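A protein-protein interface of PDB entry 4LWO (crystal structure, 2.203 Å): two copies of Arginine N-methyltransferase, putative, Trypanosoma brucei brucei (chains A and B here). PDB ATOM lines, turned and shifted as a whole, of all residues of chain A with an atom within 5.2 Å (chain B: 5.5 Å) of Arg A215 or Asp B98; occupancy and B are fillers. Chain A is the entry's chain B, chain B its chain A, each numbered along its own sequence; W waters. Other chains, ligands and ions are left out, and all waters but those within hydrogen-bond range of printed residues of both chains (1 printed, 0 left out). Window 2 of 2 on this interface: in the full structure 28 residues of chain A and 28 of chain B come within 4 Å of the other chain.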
ATOM      1  N   ASP A 212      -3.215  -7.902 -16.630  1.00  0.00           N
ATOM      2  CA  ASP A 212      -4.515  -7.977 -15.967  1.00  0.00           C
ATOM      3  C   ASP A 212      -4.375  -8.548 -14.563  1.00  0.00           C
ATOM      4  O   ASP A 212      -4.294  -9.765 -14.386  1.00  0.00           O
ATOM      5  CB  ASP A 212      -5.467  -8.856 -16.786  1.00  0.00           C
ATOM      6  CG  ASP A 212      -6.755  -9.172 -16.041  1.00  0.00           C
ATOM      7  OD1 ASP A 212      -7.183  -8.342 -15.213  1.00  0.00           O
ATOM      8  OD2 ASP A 212      -7.330 -10.255 -16.277  1.00  0.00           O
ATOM      9  N   PHE A 213      -4.349  -7.671 -13.561  1.00  0.00           N
ATOM     10  CA  PHE A 213      -4.225  -8.115 -12.179  1.00  0.00           C
ATOM     11  C   PHE A 213      -5.571  -8.037 -11.453  1.00  0.00           C
ATOM     12  O   PHE A 213      -5.609  -7.938 -10.226  1.00  0.00           O
ATOM     13  CB  PHE A 213      -3.176  -7.278 -11.429  1.00  0.00           C
ATOM     14  CG  PHE A 213      -1.753  -7.755 -11.606  1.00  0.00           C
ATOM     15  CD1 PHE A 213      -1.410  -8.619 -12.637  1.00  0.00           C
ATOM     16  CD2 PHE A 213      -0.759  -7.343 -10.717  1.00  0.00           C
ATOM     17  CE1 PHE A 213      -0.088  -9.057 -12.787  1.00  0.00           C
ATOM     18  CE2 PHE A 213       0.556  -7.771 -10.861  1.00  0.00           C
ATOM     19  CZ  PHE A 213       0.889  -8.625 -11.893  1.00  0.00           C
ATOM     20  N   SER A 214      -6.663  -8.094 -12.214  1.00  0.00           N
ATOM     21  CA  SER A 214      -8.018  -7.941 -11.670  1.00  0.00           C
ATOM     22  C   SER A 214      -8.310  -8.917 -10.533  1.00  0.00           C
ATOM     23  O   SER A 214      -8.913  -8.545  -9.533  1.00  0.00           O
ATOM     24  CB  SER A 214      -9.080  -8.073 -12.779  1.00  0.00           C
ATOM     25  OG  SER A 214      -9.090  -9.374 -13.359  1.00  0.00           O
ATOM     26  N   ARG A 215      -7.848 -10.158 -10.665  1.00  0.00           N
ATOM     27  CA  ARG A 215      -8.082 -11.158  -9.623  1.00  0.00           C
ATOM     28  C   ARG A 215      -7.597 -10.703  -8.236  1.00  0.00           C
ATOM     29  O   ARG A 215      -8.246 -10.984  -7.227  1.00  0.00           O
ATOM     30  CB  ARG A 215      -7.466 -12.509 -10.014  1.00  0.00           C
ATOM     31  CG  ARG A 215      -7.885 -13.646  -9.110  1.00  0.00           C
ATOM     32  CD  ARG A 215      -7.150 -14.917  -9.445  1.00  0.00           C
ATOM     33  NE  ARG A 215      -7.310 -15.336 -10.835  1.00  0.00           N
ATOM     34  CZ  ARG A 215      -8.346 -16.041 -11.279  1.00  0.00           C
ATOM     35  NH1 ARG A 215      -9.328 -16.380 -10.448  1.00  0.00           N
ATOM     36  NH2 ARG A 215      -8.411 -16.391 -12.555  1.00  0.00           N
ATOM     37  N   TYR A 216      -6.475  -9.982  -8.183  1.00  0.00           N
ATOM     38  CA  TYR A 216      -5.966  -9.482  -6.901  1.00  0.00           C
ATOM     39  C   TYR A 216      -6.912  -8.430  -6.288  1.00  0.00           C
ATOM     40  O   TYR A 216      -7.159  -8.421  -5.080  1.00  0.00           O
ATOM     41  CB  TYR A 216      -4.548  -8.893  -7.051  1.00  0.00           C
ATOM     42  CG  TYR A 216      -3.465  -9.905  -7.394  1.00  0.00           C
ATOM     43  CD1 TYR A 216      -3.463 -11.180  -6.833  1.00  0.00           C
ATOM     44  CD2 TYR A 216      -2.448  -9.586  -8.289  1.00  0.00           C
ATOM     45  CE1 TYR A 216      -2.486 -12.106  -7.155  1.00  0.00           C
ATOM     46  CE2 TYR A 216      -1.456 -10.514  -8.620  1.00  0.00           C
ATOM     47  CZ  TYR A 216      -1.486 -11.764  -8.050  1.00  0.00           C
ATOM     48  OH  TYR A 216      -0.514 -12.682  -8.363  1.00  0.00           O
ATOM     49  N   GLY A 217      -7.424  -7.539  -7.129  1.00  0.00           N
ATOM     50  CA  GLY A 217      -8.350  -6.507  -6.689  1.00  0.00           C
ATOM     51  C   GLY A 217      -9.619  -7.045  -6.048  1.00  0.00           C
ATOM     52  O   GLY A 217     -10.122  -6.485  -5.071  1.00  0.00           O
ATOM     53  N   ARG A 218     -10.141  -8.137  -6.590  1.00  0.00           N
ATOM     54  CA  ARG A 218     -11.332  -8.749  -6.021  1.00  0.00           C
ATOM     55  C   ARG A 218     -11.015  -9.360  -4.670  1.00  0.00           C
ATOM     56  O   ARG A 218     -11.787  -9.198  -3.726  1.00  0.00           O
ATOM     57  CB  ARG A 218     -11.920  -9.779  -6.980  1.00  0.00           C
ATOM     58  CG  ARG A 218     -12.447  -9.145  -8.262  1.00  0.00           C
ATOM     59  CD  ARG A 218     -13.168 -10.151  -9.165  1.00  0.00           C
ATOM     60  NE  ARG A 218     -12.284 -10.660 -10.206  1.00  0.00           N
ATOM     61  CZ  ARG A 218     -11.840 -11.907 -10.261  1.00  0.00           C
ATOM     62  NH1 ARG A 218     -12.214 -12.784  -9.337  1.00  0.00           N
ATOM     63  NH2 ARG A 218     -11.029 -12.277 -11.245  1.00  0.00           N
ATOM     64  N   ILE A 219      -9.867 -10.041  -4.578  1.00  0.00           N
ATOM     65  CA  ILE A 219      -9.419 -10.629  -3.322  1.00  0.00           C
ATOM     66  C   ILE A 219      -9.350  -9.566  -2.243  1.00  0.00           C
ATOM     67  O   ILE A 219      -9.908  -9.720  -1.158  1.00  0.00           O
ATOM     68  CB  ILE A 219      -8.015 -11.244  -3.460  1.00  0.00           C
ATOM     69  CG1 ILE A 219      -8.094 -12.565  -4.207  1.00  0.00           C
ATOM     70  CG2 ILE A 219      -7.397 -11.484  -2.088  1.00  0.00           C
ATOM     71  CD1 ILE A 219      -8.980 -13.552  -3.506  1.00  0.00           C
ATOM     72  N   PHE B  91      -3.206 -17.741  -5.725  1.00  0.00           N
ATOM     73  CA  PHE B  91      -3.837 -16.714  -6.550  1.00  0.00           C
ATOM     74  C   PHE B  91      -2.954 -16.256  -7.719  1.00  0.00           C
ATOM     75  O   PHE B  91      -3.455 -16.002  -8.814  1.00  0.00           O
ATOM     76  CB  PHE B  91      -4.267 -15.536  -5.678  1.00  0.00           C
ATOM     77  CG  PHE B  91      -5.328 -15.895  -4.667  1.00  0.00           C
ATOM     78  CD1 PHE B  91      -6.602 -16.276  -5.081  1.00  0.00           C
ATOM     79  CD2 PHE B  91      -5.064 -15.837  -3.309  1.00  0.00           C
ATOM     80  CE1 PHE B  91      -7.585 -16.606  -4.157  1.00  0.00           C
ATOM     81  CE2 PHE B  91      -6.044 -16.158  -2.379  1.00  0.00           C
ATOM     82  CZ  PHE B  91      -7.304 -16.548  -2.808  1.00  0.00           C
ATOM     83  N   ILE B  93      -0.904 -18.103  -9.391  1.00  0.00           N
ATOM     84  CA  ILE B  93      -1.117 -19.110 -10.435  1.00  0.00           C
ATOM     85  C   ILE B  93      -2.324 -18.716 -11.314  1.00  0.00           C
ATOM     86  O   ILE B  93      -2.293 -18.868 -12.538  1.00  0.00           O
ATOM     87  CB  ILE B  93      -1.314 -20.509  -9.811  1.00  0.00           C
ATOM     88  CG1 ILE B  93       0.017 -21.021  -9.258  1.00  0.00           C
ATOM     89  CG2 ILE B  93      -1.917 -21.494 -10.830  1.00  0.00           C
ATOM     90  CD1 ILE B  93      -0.085 -22.241  -8.351  1.00  0.00           C
ATOM     91  N   GLY B  94      -3.368 -18.171 -10.685  1.00  0.00           N
ATOM     92  CA  GLY B  94      -4.548 -17.729 -11.410  1.00  0.00           C
ATOM     93  C   GLY B  94      -4.251 -16.532 -12.289  1.00  0.00           C
ATOM     94  O   GLY B  94      -4.632 -16.488 -13.469  1.00  0.00           O
ATOM     95  N   VAL B  95      -3.555 -15.556 -11.719  1.00  0.00           N
ATOM     96  CA  VAL B  95      -3.177 -14.372 -12.481  1.00  0.00           C
ATOM     97  C   VAL B  95      -2.243 -14.699 -13.650  1.00  0.00           C
ATOM     98  O   VAL B  95      -2.374 -14.107 -14.735  1.00  0.00           O
ATOM     99  CB  VAL B  95      -2.553 -13.286 -11.593  1.00  0.00           C
ATOM    100  CG1 VAL B  95      -2.167 -12.070 -12.438  1.00  0.00           C
ATOM    101  CG2 VAL B  95      -3.523 -12.881 -10.473  1.00  0.00           C
ATOM    102  N   VAL B  96      -1.306 -15.630 -13.430  1.00  0.00           N
ATOM    103  CA  VAL B  96      -0.427 -16.097 -14.508  1.00  0.00           C
ATOM    104  C   VAL B  96      -1.292 -16.663 -15.640  1.00  0.00           C
ATOM    105  O   VAL B  96      -1.086 -16.358 -16.815  1.00  0.00           O
ATOM    106  CB  VAL B  96       0.587 -17.186 -14.025  1.00  0.00           C
ATOM    107  CG1 VAL B  96       1.130 -17.966 -15.200  1.00  0.00           C
ATOM    108  CG2 VAL B  96       1.746 -16.569 -13.221  1.00  0.00           C
ATOM    109  N   GLU B  97      -2.270 -17.485 -15.277  1.00  0.00           N
ATOM    110  CA  GLU B  97      -3.208 -18.029 -16.260  1.00  0.00           C
ATOM    111  C   GLU B  97      -4.002 -16.909 -16.950  1.00  0.00           C
ATOM    112  O   GLU B  97      -4.075 -16.866 -18.184  1.00  0.00           O
ATOM    113  CB  GLU B  97      -4.128 -19.071 -15.608  1.00  0.00           C
ATOM    114  CG  GLU B  97      -5.152 -19.724 -16.541  1.00  0.00           C
ATOM    115  CD  GLU B  97      -4.541 -20.266 -17.826  1.00  0.00           C
ATOM    116  OE1 GLU B  97      -4.621 -19.569 -18.859  1.00  0.00           O
ATOM    117  OE2 GLU B  97      -3.982 -21.385 -17.814  1.00  0.00           O
ATOM    118  N   ASP B  98      -4.556 -15.983 -16.169  1.00  0.00           N
ATOM    119  CA  ASP B  98      -5.287 -14.847 -16.732  1.00  0.00           C
ATOM    120  C   ASP B  98      -4.486 -14.023 -17.758  1.00  0.00           C
ATOM    121  O   ASP B  98      -5.070 -13.280 -18.547  1.00  0.00           O
ATOM    122  CB  ASP B  98      -5.724 -13.871 -15.631  1.00  0.00           C
ATOM    123  CG  ASP B  98      -6.682 -14.478 -14.634  1.00  0.00           C
ATOM    124  OD1 ASP B  98      -7.335 -15.494 -14.958  1.00  0.00           O
ATOM    125  OD2 ASP B  98      -6.779 -13.916 -13.511  1.00  0.00           O
ATOM    126  N   ASN B  99      -3.158 -14.101 -17.724  1.00  0.00           N
ATOM    127  CA  ASN B  99      -2.359 -13.319 -18.667  1.00  0.00           C
ATOM    128  C   ASN B  99      -1.700 -14.250 -19.673  1.00  0.00           C
ATOM    129  O   ASN B  99      -0.760 -13.869 -20.371  1.00  0.00           O
ATOM    130  CB  ASN B  99      -1.319 -12.460 -17.940  1.00  0.00           C
ATOM    131  CG  ASN B  99      -1.957 -11.344 -17.092  1.00  0.00           C
ATOM    132  OD1 ASN B  99      -2.172 -10.227 -17.570  1.00  0.00           O
ATOM    133  ND2 ASN B  99      -2.250 -11.647 -15.828  1.00  0.00           N
ATOM    134  N   ASP B 100      -2.194 -15.485 -19.705  1.00  0.00           N
ATOM    135  CA  ASP B 100      -1.789 -16.501 -20.686  1.00  0.00           C
ATOM    136  C   ASP B 100      -0.293 -16.799 -20.630  1.00  0.00           C
ATOM    137  O   ASP B 100       0.409 -16.663 -21.630  1.00  0.00           O
ATOM    138  CB  ASP B 100      -2.191 -16.063 -22.100  1.00  0.00           C
HETATM  139  O   HOH W   1      -6.203 -11.414 -12.822  1.00  0.00           O
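N of Asp A212 sits at hydrogen-bond distance from OD1 of Asn B99, 2.7 Å away. The side-chain carboxylate (OD1) of Asp B98 is in salt-bridge range of the guanidinium group (NH2) of Arg A215, 2.8 Å away.
The side-chain carboxylate of Asp A212 sits at hydrogen-bond distance from the side-chain hydroxyl of Ser A214 (2.9 Å). The backbone carbonyl oxygen (O) of Val B95 is in hydrogen-bond range of the side-chain amide nitrogen (ND2) of Asn B99 (2.7 Å).
Among the printed residues, merely in contact across the chains: Asp A212 with Val B95, Phe A213 with Val B95, Arg A215 with Phe B91, Arg A215 with Gly B94, Arg A215 with Val B95, Tyr A216 with Val B95 and Ile A219 with Phe B91.
Printed residues of chain B within 4 Å of Arg A215: Phe B91 (3.9 Å), Gly B94 (3.6 Å), Val B95 (3.9 Å) and Asp B98 (2.8 Å). Printed residues of chain B within 4 Å of Phe A213: Val B95. Printed residues of chain A within 4 Å of Gly B94: Arg A215 (3.6 Å). Printed residues of chain A within 4 Å of Asn B99: Asp A212 (2.7 Å). Of the printed residues of chain A, Val B95 touches Asp A212, Phe A213, Arg A215 and Tyr A216. Glu B97 touches none of the printed residues of chain A. The nearest printed residue of chain A that does not touch Asp B98 is Asp A212 (4.01 Å). The nearest printed residue of chain B that does not touch Phe A213 is Asn B99 (4.5 Å).
Of the 9 printed residues of chain B, 5 touch a printed residue of chain A. Printed residues of chain B that touch a printed residue of chain A: Phe B91, Gly B94, Val B95, Asp B98 and Asn B99. Along chain A the printed residues that touch a printed residue of chain B span positions 212 to 219.
No position is printed for both chains. Of the 9 pairs that touch across the chains among the printed residues, none has its exchanged pair printed and touching as well.
Water W1 lies within hydrogen-bond range of the side-chain carboxylate of Asp B98 (2.7 Å), the backbone carbonyl oxygen of Asp A212 (3.0 Å), the backbone NH of Arg A215 (3.0 Å) and the backbone NH of Ser A214 (3.4 Å).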
